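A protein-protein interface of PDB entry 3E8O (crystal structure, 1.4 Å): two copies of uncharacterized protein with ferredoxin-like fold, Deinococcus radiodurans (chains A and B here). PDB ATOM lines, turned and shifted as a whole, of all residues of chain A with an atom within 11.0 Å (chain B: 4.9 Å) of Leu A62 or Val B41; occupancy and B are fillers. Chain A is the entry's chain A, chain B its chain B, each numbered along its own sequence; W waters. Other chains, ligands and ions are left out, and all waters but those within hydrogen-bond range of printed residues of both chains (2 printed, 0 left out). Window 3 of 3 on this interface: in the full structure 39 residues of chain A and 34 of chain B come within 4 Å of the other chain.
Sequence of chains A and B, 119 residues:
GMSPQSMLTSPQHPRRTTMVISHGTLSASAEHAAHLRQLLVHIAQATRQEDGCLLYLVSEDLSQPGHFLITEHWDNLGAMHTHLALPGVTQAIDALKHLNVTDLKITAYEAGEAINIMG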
ATOM      1  N   LEU A  26     -10.539  15.361 -11.117  1.00  0.00           N
ATOM      2  CA  LEU A  26      -9.081  15.546 -11.000  1.00  0.00           C
ATOM      3  C   LEU A  26      -8.384  14.501 -11.843  1.00  0.00           C
ATOM      4  O   LEU A  26      -8.990  13.465 -12.161  1.00  0.00           O
ATOM      5  CB  LEU A  26      -8.574  15.460  -9.564  1.00  0.00           C
ATOM      6  CG  LEU A  26      -8.661  14.140  -8.800  1.00  0.00           C
ATOM      7  CD1 LEU A  26      -7.795  14.256  -7.518  1.00  0.00           C
ATOM      8  CD2 LEU A  26     -10.120  13.685  -8.504  1.00  0.00           C
ATOM      9  N   ARG A  37      -4.519   6.948  -6.968  1.00  0.00           N
ATOM     10  CA  ARG A  37      -5.591   5.987  -6.699  1.00  0.00           C
ATOM     11  C   ARG A  37      -5.545   5.570  -5.245  1.00  0.00           C
ATOM     12  O   ARG A  37      -6.544   5.464  -4.584  1.00  0.00           O
ATOM     13  CB  ARG A  37      -5.523   4.745  -7.616  1.00  0.00           C
ATOM     14  CG  ARG A  37      -5.756   5.039  -9.074  1.00  0.00           C
ATOM     15  CD  ARG A  37      -5.778   3.773  -9.922  1.00  0.00           C
ATOM     16  NE  ARG A  37      -5.787   4.070 -11.334  1.00  0.00           N
ATOM     17  CZ  ARG A  37      -4.730   4.159 -12.128  1.00  0.00           C
ATOM     18  NH1 ARG A  37      -3.525   3.822 -11.713  1.00  0.00           N
ATOM     19  NH2 ARG A  37      -4.891   4.565 -13.358  1.00  0.00           N
ATOM     20  N   VAL A  58     -14.981   7.282  -4.883  1.00  0.00           N
ATOM     21  CA  VAL A  58     -13.890   7.706  -5.718  1.00  0.00           C
ATOM     22  C   VAL A  58     -13.803   6.717  -6.876  1.00  0.00           C
ATOM     23  O   VAL A  58     -13.859   5.497  -6.671  1.00  0.00           O
ATOM     24  CB  VAL A  58     -12.573   7.824  -4.960  1.00  0.00           C
ATOM     25  CG1 VAL A  58     -12.638   8.978  -3.942  1.00  0.00           C
ATOM     26  CG2 VAL A  58     -12.094   6.485  -4.218  1.00  0.00           C
ATOM     27  N   SER A  59     -13.761   7.232  -8.100  1.00  0.00           N
ATOM     28  CA  SER A  59     -13.873   6.373  -9.299  1.00  0.00           C
ATOM     29  C   SER A  59     -13.010   6.891 -10.425  1.00  0.00           C
ATOM     30  O   SER A  59     -12.586   8.037 -10.430  1.00  0.00           O
ATOM     31  CB  SER A  59     -15.359   6.233  -9.708  1.00  0.00           C
ATOM     32  OG  SER A  59     -15.934   7.488 -10.088  1.00  0.00           O
ATOM     33  N   GLU A  60     -12.791   6.029 -11.393  1.00  0.00           N
ATOM     34  CA  GLU A  60     -11.963   6.348 -12.558  1.00  0.00           C
ATOM     35  C   GLU A  60     -12.785   6.263 -13.833  1.00  0.00           C
ATOM     36  O   GLU A  60     -13.519   5.310 -14.064  1.00  0.00           O
ATOM     37  CB  GLU A  60     -10.754   5.399 -12.650  1.00  0.00           C
ATOM     38  CG  GLU A  60      -9.738   5.823 -13.681  1.00  0.00           C
ATOM     39  CD  GLU A  60      -8.405   5.093 -13.585  1.00  0.00           C
ATOM     40  OE1 GLU A  60      -8.267   4.249 -12.686  1.00  0.00           O
ATOM     41  OE2 GLU A  60      -7.477   5.418 -14.402  1.00  0.00           O
ATOM     42  N   ASP A  61     -12.675   7.320 -14.616  1.00  0.00           N
ATOM     43  CA  ASP A  61     -13.420   7.511 -15.854  1.00  0.00           C
ATOM     44  C   ASP A  61     -13.075   6.405 -16.839  1.00  0.00           C
ATOM     45  O   ASP A  61     -11.898   6.285 -17.222  1.00  0.00           O
ATOM     46  CB  ASP A  61     -13.077   8.917 -16.427  1.00  0.00           C
ATOM     47  CG  ASP A  61     -13.966   9.322 -17.589  1.00  0.00           C
ATOM     48  OD1 ASP A  61     -14.520   8.436 -18.240  1.00  0.00           O
ATOM     49  OD2 ASP A  61     -14.045  10.533 -17.842  1.00  0.00           O
ATOM     50  N   LEU A  62     -14.055   5.595 -17.233  1.00  0.00           N
ATOM     51  CA  LEU A  62     -13.813   4.504 -18.180  1.00  0.00           C
ATOM     52  C   LEU A  62     -13.352   5.063 -19.550  1.00  0.00           C
ATOM     53  O   LEU A  62     -12.723   4.344 -20.299  1.00  0.00           O
ATOM     54  CB  LEU A  62     -15.093   3.643 -18.387  1.00  0.00           C
ATOM     55  CG  LEU A  62     -15.538   2.813 -17.215  1.00  0.00           C
ATOM     56  CD1 LEU A  62     -16.852   2.151 -17.594  1.00  0.00           C
ATOM     57  CD2 LEU A  62     -14.483   1.770 -16.884  1.00  0.00           C
ATOM     58  N   SER A  63     -13.797   6.299 -19.852  1.00  0.00           N
ATOM     59  CA  SER A  63     -13.589   7.018 -21.146  1.00  0.00           C
ATOM     60  C   SER A  63     -12.246   7.740 -21.169  1.00  0.00           C
ATOM     61  O   SER A  63     -11.791   8.152 -22.243  1.00  0.00           O
ATOM     62  CB  SER A  63     -14.750   8.019 -21.426  1.00  0.00           C
ATOM     63  OG  SER A  63     -16.081   7.406 -21.447  1.00  0.00           O
ATOM     64  N   GLN A  64     -11.584   7.829 -20.017  1.00  0.00           N
ATOM     65  CA  GLN A  64     -10.307   8.559 -19.855  1.00  0.00           C
ATOM     66  C   GLN A  64      -9.454   8.105 -18.680  1.00  0.00           C
ATOM     67  O   GLN A  64      -9.522   8.665 -17.586  1.00  0.00           O
ATOM     68  CB  GLN A  64     -10.564  10.034 -19.588  1.00  0.00           C
ATOM     69  CG  GLN A  64     -11.387  10.816 -20.518  1.00  0.00           C
ATOM     70  CD  GLN A  64     -11.248  12.274 -20.144  1.00  0.00           C
ATOM     71  OE1 GLN A  64     -10.243  12.898 -20.465  1.00  0.00           O
ATOM     72  NE2 GLN A  64     -12.221  12.808 -19.409  1.00  0.00           N
ATOM     73  N   PRO A  65      -8.607   7.110 -18.883  1.00  0.00           N
ATOM     74  CA  PRO A  65      -7.714   6.601 -17.852  1.00  0.00           C
ATOM     75  C   PRO A  65      -6.900   7.718 -17.240  1.00  0.00           C
ATOM     76  O   PRO A  65      -6.495   8.665 -17.937  1.00  0.00           O
ATOM     77  CB  PRO A  65      -6.830   5.621 -18.609  1.00  0.00           C
ATOM     78  CG  PRO A  65      -7.691   5.189 -19.726  1.00  0.00           C
ATOM     79  CD  PRO A  65      -8.433   6.382 -20.160  1.00  0.00           C
ATOM     80  N   GLY A  66      -6.777   7.668 -15.914  1.00  0.00           N
ATOM     81  CA  GLY A  66      -6.016   8.658 -15.163  1.00  0.00           C
ATOM     82  C   GLY A  66      -6.832   9.869 -14.791  1.00  0.00           C
ATOM     83  O   GLY A  66      -6.312  10.790 -14.181  1.00  0.00           O
ATOM     84  N   HIS A  67      -8.114   9.844 -15.144  1.00  0.00           N
ATOM     85  CA  HIS A  67      -9.089  10.929 -14.798  1.00  0.00           C
ATOM     86  C   HIS A  67     -10.079  10.328 -13.818  1.00  0.00           C
ATOM     87  O   HIS A  67     -10.649   9.270 -14.066  1.00  0.00           O
ATOM     88  CB  HIS A  67      -9.752  11.473 -16.049  1.00  0.00           C
ATOM     89  CG  HIS A  67      -8.796  12.177 -16.957  1.00  0.00           C
ATOM     90  ND1 HIS A  67      -8.864  13.526 -17.184  1.00  0.00           N
ATOM     91  CD2 HIS A  67      -7.717  11.726 -17.639  1.00  0.00           C
ATOM     92  CE1 HIS A  67      -7.891  13.877 -18.011  1.00  0.00           C
ATOM     93  NE2 HIS A  67      -7.189  12.796 -18.318  1.00  0.00           N
ATOM     94  N   PHE A  68     -10.263  11.041 -12.715  1.00  0.00           N
ATOM     95  CA  PHE A  68     -11.006  10.539 -11.558  1.00  0.00           C
ATOM     96  C   PHE A  68     -12.135  11.468 -11.181  1.00  0.00           C
ATOM     97  O   PHE A  68     -12.159  12.659 -11.502  1.00  0.00           O
ATOM     98  CB  PHE A  68     -10.042  10.367 -10.365  1.00  0.00           C
ATOM     99  CG  PHE A  68      -8.869   9.451 -10.663  1.00  0.00           C
ATOM    100  CD1 PHE A  68      -9.007   8.087 -10.622  1.00  0.00           C
ATOM    101  CD2 PHE A  68      -7.641   9.969 -11.078  1.00  0.00           C
ATOM    102  CE1 PHE A  68      -7.986   7.256 -10.955  1.00  0.00           C
ATOM    103  CE2 PHE A  68      -6.616   9.129 -11.416  1.00  0.00           C
ATOM    104  CZ  PHE A  68      -6.789   7.774 -11.355  1.00  0.00           C
ATOM    105  N   LEU A  69     -13.085  10.843 -10.495  1.00  0.00           N
ATOM    106  CA  LEU A  69     -14.284  11.491  -9.998  1.00  0.00           C
ATOM    107  C   LEU A  69     -14.416  11.244  -8.496  1.00  0.00           C
ATOM    108  O   LEU A  69     -14.137  10.143  -8.010  1.00  0.00           O
ATOM    109  CB  LEU A  69     -15.525  10.933 -10.742  1.00  0.00           C
ATOM    110  CG  LEU A  69     -16.943  11.472 -10.509  1.00  0.00           C
ATOM    111  CD1 LEU A  69     -17.085  12.944 -10.925  1.00  0.00           C
ATOM    112  CD2 LEU A  69     -17.991  10.607 -11.270  1.00  0.00           C
ATOM    113  N   ARG B  37     -18.183  -2.636 -19.223  1.00  0.00           N
ATOM    114  CA  ARG B  37     -17.385  -1.411 -19.455  1.00  0.00           C
ATOM    115  C   ARG B  37     -17.595  -0.893 -20.876  1.00  0.00           C
ATOM    116  O   ARG B  37     -17.766   0.309 -21.093  1.00  0.00           O
ATOM    117  CB  ARG B  37     -15.882  -1.666 -19.222  1.00  0.00           C
ATOM    118  CG  ARG B  37     -15.537  -2.004 -17.766  1.00  0.00           C
ATOM    119  CD  ARG B  37     -14.027  -2.199 -17.538  1.00  0.00           C
ATOM    120  NE  ARG B  37     -13.787  -2.639 -16.185  1.00  0.00           N
ATOM    121  CZ  ARG B  37     -13.709  -3.896 -15.772  1.00  0.00           C
ATOM    122  NH1 ARG B  37     -13.681  -4.882 -16.640  1.00  0.00           N
ATOM    123  NH2 ARG B  37     -13.692  -4.150 -14.475  1.00  0.00           N
ATOM    124  N   GLN B  38     -17.537  -1.797 -21.868  1.00  0.00           N
ATOM    125  CA  GLN B  38     -17.719  -1.375 -23.261  1.00  0.00           C
ATOM    126  C   GLN B  38     -19.102  -0.804 -23.512  1.00  0.00           C
ATOM    127  O   GLN B  38     -19.266   0.187 -24.176  1.00  0.00           O
ATOM    128  CB  GLN B  38     -17.403  -2.535 -24.192  1.00  0.00           C
ATOM    129  CG  GLN B  38     -17.184  -2.026 -25.603  1.00  0.00           C
ATOM    130  CD  GLN B  38     -15.878  -1.192 -25.737  1.00  0.00           C
ATOM    131  OE1 GLN B  38     -14.748  -1.674 -25.506  1.00  0.00           O
ATOM    132  NE2 GLN B  38     -16.029   0.024 -26.181  1.00  0.00           N
ATOM    133  N   LEU B  39     -20.091  -1.451 -22.948  1.00  0.00           N
ATOM    134  CA  LEU B  39     -21.482  -0.958 -23.027  1.00  0.00           C
ATOM    135  C   LEU B  39     -21.616   0.438 -22.453  1.00  0.00           C
ATOM    136  O   LEU B  39     -22.242   1.304 -23.036  1.00  0.00           O
ATOM    137  CB  LEU B  39     -22.469  -1.907 -22.352  1.00  0.00           C
ATOM    138  CG  LEU B  39     -23.941  -1.542 -22.339  1.00  0.00           C
ATOM    139  CD1 LEU B  39     -24.449  -1.382 -23.793  1.00  0.00           C
ATOM    140  CD2 LEU B  39     -24.720  -2.617 -21.590  1.00  0.00           C
ATOM    141  N   LEU B  40     -21.022   0.641 -21.280  1.00  0.00           N
ATOM    142  CA  LEU B  40     -21.128   1.934 -20.592  1.00  0.00           C
ATOM    143  C   LEU B  40     -20.470   3.032 -21.422  1.00  0.00           C
ATOM    144  O   LEU B  40     -21.007   4.129 -21.558  1.00  0.00           O
ATOM    145  CB  LEU B  40     -20.511   1.868 -19.191  1.00  0.00           C
ATOM    146  CG  LEU B  40     -21.393   1.095 -18.200  1.00  0.00           C
ATOM    147  CD1 LEU B  40     -20.630   0.814 -16.881  1.00  0.00           C
ATOM    148  CD2 LEU B  40     -22.731   1.818 -17.919  1.00  0.00           C
ATOM    149  N   VAL B  41     -19.287   2.746 -21.965  1.00  0.00           N
ATOM    150  CA  VAL B  41     -18.566   3.739 -22.776  1.00  0.00           C
ATOM    151  C   VAL B  41     -19.391   4.094 -24.030  1.00  0.00           C
ATOM    152  O   VAL B  41     -19.486   5.232 -24.434  1.00  0.00           O
ATOM    153  CB  VAL B  41     -17.112   3.303 -23.107  1.00  0.00           C
ATOM    154  CG1 VAL B  41     -16.531   4.131 -24.249  1.00  0.00           C
ATOM    155  CG2 VAL B  41     -16.249   3.344 -21.821  1.00  0.00           C
ATOM    156  N   HIS B  42     -20.002   3.077 -24.610  1.00  0.00           N
ATOM    157  CA  HIS B  42     -20.811   3.260 -25.809  1.00  0.00           C
ATOM    158  C   HIS B  42     -22.009   4.161 -25.499  1.00  0.00           C
ATOM    159  O   HIS B  42     -22.279   5.114 -26.221  1.00  0.00           O
ATOM    160  CB  HIS B  42     -21.261   1.892 -26.367  1.00  0.00           C
ATOM    161  CG  HIS B  42     -22.090   1.967 -27.610  1.00  0.00           C
ATOM    162  ND1 HIS B  42     -23.464   2.079 -27.585  1.00  0.00           N
ATOM    163  CD2 HIS B  42     -21.735   1.928 -28.913  1.00  0.00           C
ATOM    164  CE1 HIS B  42     -23.923   2.119 -28.829  1.00  0.00           C
ATOM    165  NE2 HIS B  42     -22.896   2.006 -29.652  1.00  0.00           N
ATOM    166  N   ILE B  43     -22.733   3.857 -24.430  1.00  0.00           N
ATOM    167  CA  ILE B  43     -23.907   4.639 -24.047  1.00  0.00           C
ATOM    168  C   ILE B  43     -23.518   6.066 -23.720  1.00  0.00           C
ATOM    169  O   ILE B  43     -24.239   6.996 -24.047  1.00  0.00           O
ATOM    170  CB  ILE B  43     -24.670   4.046 -22.822  1.00  0.00           C
ATOM    171  CG1 ILE B  43     -25.255   2.697 -23.180  1.00  0.00           C
ATOM    172  CG2 ILE B  43     -25.784   4.984 -22.344  1.00  0.00           C
ATOM    173  CD1 ILE B  43     -25.599   1.909 -21.908  1.00  0.00           C
ATOM    174  N   ALA B  44     -22.382   6.245 -23.055  1.00  0.00           N
ATOM    175  CA  ALA B  44     -21.942   7.593 -22.699  1.00  0.00           C
ATOM    176  C   ALA B  44     -21.666   8.420 -23.963  1.00  0.00           C
ATOM    177  O   ALA B  44     -22.074   9.557 -24.045  1.00  0.00           O
ATOM    178  CB  ALA B  44     -20.709   7.513 -21.844  1.00  0.00           C
ATOM    179  N   GLN B  45     -21.007   7.811 -24.945  1.00  0.00           N
ATOM    180  CA  GLN B  45     -20.651   8.507 -26.188  1.00  0.00           C
ATOM    181  C   GLN B  45     -21.900   8.958 -26.921  1.00  0.00           C
ATOM    182  O   GLN B  45     -21.984  10.054 -27.450  1.00  0.00           O
ATOM    183  CB  GLN B  45     -19.787   7.602 -27.094  1.00  0.00           C
ATOM    184  CG  GLN B  45     -19.217   8.335 -28.321  1.00  0.00           C
ATOM    185  N   VAL B  58     -19.172   7.777 -17.149  1.00  0.00           N
ATOM    186  CA  VAL B  58     -19.204   6.404 -16.688  1.00  0.00           C
ATOM    187  C   VAL B  58     -17.862   6.064 -16.057  1.00  0.00           C
ATOM    188  O   VAL B  58     -16.827   6.318 -16.644  1.00  0.00           O
ATOM    189  CB  VAL B  58     -19.620   5.420 -17.797  1.00  0.00           C
ATOM    190  CG1 VAL B  58     -21.127   5.641 -18.116  1.00  0.00           C
ATOM    191  CG2 VAL B  58     -18.722   5.527 -19.057  1.00  0.00           C
ATOM    192  N   SER B  59     -17.883   5.551 -14.824  1.00  0.00           N
ATOM    193  CA  SER B  59     -16.642   5.363 -14.068  1.00  0.00           C
ATOM    194  C   SER B  59     -16.716   4.095 -13.223  1.00  0.00           C
ATOM    195  O   SER B  59     -17.772   3.539 -13.017  1.00  0.00           O
ATOM    196  CB  SER B  59     -16.375   6.617 -13.221  1.00  0.00           C
ATOM    197  OG  SER B  59     -17.393   6.833 -12.245  1.00  0.00           O
ATOM    198  N   GLU B  60     -15.545   3.651 -12.802  1.00  0.00           N
ATOM    199  CA  GLU B  60     -15.380   2.460 -12.006  1.00  0.00           C
ATOM    200  C   GLU B  60     -14.833   2.823 -10.640  1.00  0.00           C
ATOM    201  O   GLU B  60     -13.819   3.511 -10.516  1.00  0.00           O
ATOM    202  CB  GLU B  60     -14.486   1.451 -12.754  1.00  0.00           C
ATOM    203  CG  GLU B  60     -14.450   0.082 -12.070  1.00  0.00           C
ATOM    204  CD  GLU B  60     -13.876  -1.028 -12.924  1.00  0.00           C
ATOM    205  OE1 GLU B  60     -13.484  -0.758 -14.073  1.00  0.00           O
ATOM    206  OE2 GLU B  60     -13.790  -2.166 -12.400  1.00  0.00           O
ATOM    207  N   PHE B  68     -19.691   0.129 -10.920  1.00  0.00           N
ATOM    208  CA  PHE B  68     -19.721   1.280 -11.804  1.00  0.00           C
ATOM    209  C   PHE B  68     -20.663   2.356 -11.364  1.00  0.00           C
ATOM    210  O   PHE B  68     -21.629   2.099 -10.667  1.00  0.00           O
ATOM    211  CB  PHE B  68     -20.010   0.805 -13.255  1.00  0.00           C
ATOM    212  CG  PHE B  68     -19.031  -0.213 -13.712  1.00  0.00           C
ATOM    213  CD1 PHE B  68     -17.806   0.157 -14.188  1.00  0.00           C
ATOM    214  CD2 PHE B  68     -19.321  -1.560 -13.613  1.00  0.00           C
ATOM    215  CE1 PHE B  68     -16.874  -0.818 -14.575  1.00  0.00           C
ATOM    216  CE2 PHE B  68     -18.398  -2.530 -14.029  1.00  0.00           C
ATOM    217  CZ  PHE B  68     -17.174  -2.136 -14.486  1.00  0.00           C
HETATM  218  O   HOH W   1     -17.487   7.195 -23.761  1.00  0.00           O
HETATM  219  O   HOH W   2     -17.130   8.606 -19.061  1.00  0.00           O
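The side-chain hydroxyl (OG) of Ser B59 sits at hydrogen-bond distance from the side-chain hydroxyl (OG) of Ser A59 (2.7 Å).
O of Glu B60 lies within hydrogen-bond range of N of Glu A60, at 2.9 Å.
N of Leu A62 is in hydrogen-bond range of O of Val B58 (2.9 Å).
OE1 of Glu A60 is in salt-bridge range of NE of Arg A37, at 2.8 Å.
N of Gly A66 lies within hydrogen-bond range of OE2 of Glu A60.
The backbone NH of Ser A63 lies within hydrogen-bond range of the side-chain carboxylate of Asp A61 (2.8 Å).
OD2 of Asp A61 is in hydrogen-bond range of NE2 of Gln A64 (3.3 Å).
O of His A67 is in hydrogen-bond range of N of Asp A61 (2.9 Å).
The guanidinium group (NE) of Arg B37 is in salt-bridge range of the side-chain carboxylate (OE1) of Glu B60 (2.8 Å).
Among the printed residues, pairs that only touch across the chains: Ser A59 with Glu B60 (3.1 Å), Glu A60 with Ser B59 (3.1 Å), Asp A61 with Val B58 (3.5 Å), Leu A62 with Val B41 (3.6 Å), Leu A62 with Glu B60 (3.9 Å) and Leu A69 with Ser B59 (3.9 Å).
Printed residues of chain B within 4 Å of Leu A62: Val B41, Val B58 and Glu B60.
Val B41 touches just one residue of chain A: Leu A62 (3.6 Å).
No residue of chain A comes within 4 Å of Gln B38.
His B42 touches none of the printed residues of chain A.
No residue of chain A comes within 4 Å of Ile B43.
No residue of chain A comes within 4 Å of Ala B44.
No residue of chain A comes within 4 Å of Gln B45.
Of the printed residues of chain A, Ser B59 touches Ser A59, Glu A60 and Leu A69.
Printed residues of chain B within 4 Å of Ser A59: Ser B59 and Glu B60.
Arg B37 touches none of the printed residues of chain A.
The nearest printed residue of chain B that does not touch Leu A62 is Leu B40 (4.002 Å).
The nearest residue of chain A that does not touch Val B41 is Ser A63 (4.1 Å).
Hydrophobic or aromatic side chains of chain A within 4 Å of the printed part of chain B: Leu A62 and Leu A69.
Hydrophobic or aromatic side chains of chain B that line the printed part of chain A: Val B41.
Among the printed residues, no Asp or Glu carboxylate lies within 4 Å of a Lys or Arg side-chain nitrogen of the other chain.
Ser B59 touches its own counterpart, Ser A59.
Ser A59 touches Glu B60, and with the chains exchanged Glu A60 touches Ser B59.
Glu A60 touches its own counterpart, Glu B60.
Positions printed for both chains: 37, 58, 59, 60 and 68.
Of the 9 pairs that touch across the chains among the printed residues, 4 have their exchanged pair printed and touching as well.
Water W1 lies within hydrogen-bond range of OG of Ser A63 (2.7 Å) and O of Val B41 (2.9 Å).
Water W2 lies within hydrogen-bond range of OD1 of Asp A61 (2.7 Å), OG of Ser A63 (2.9 Å) and N of Val B58 (2.9 Å).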
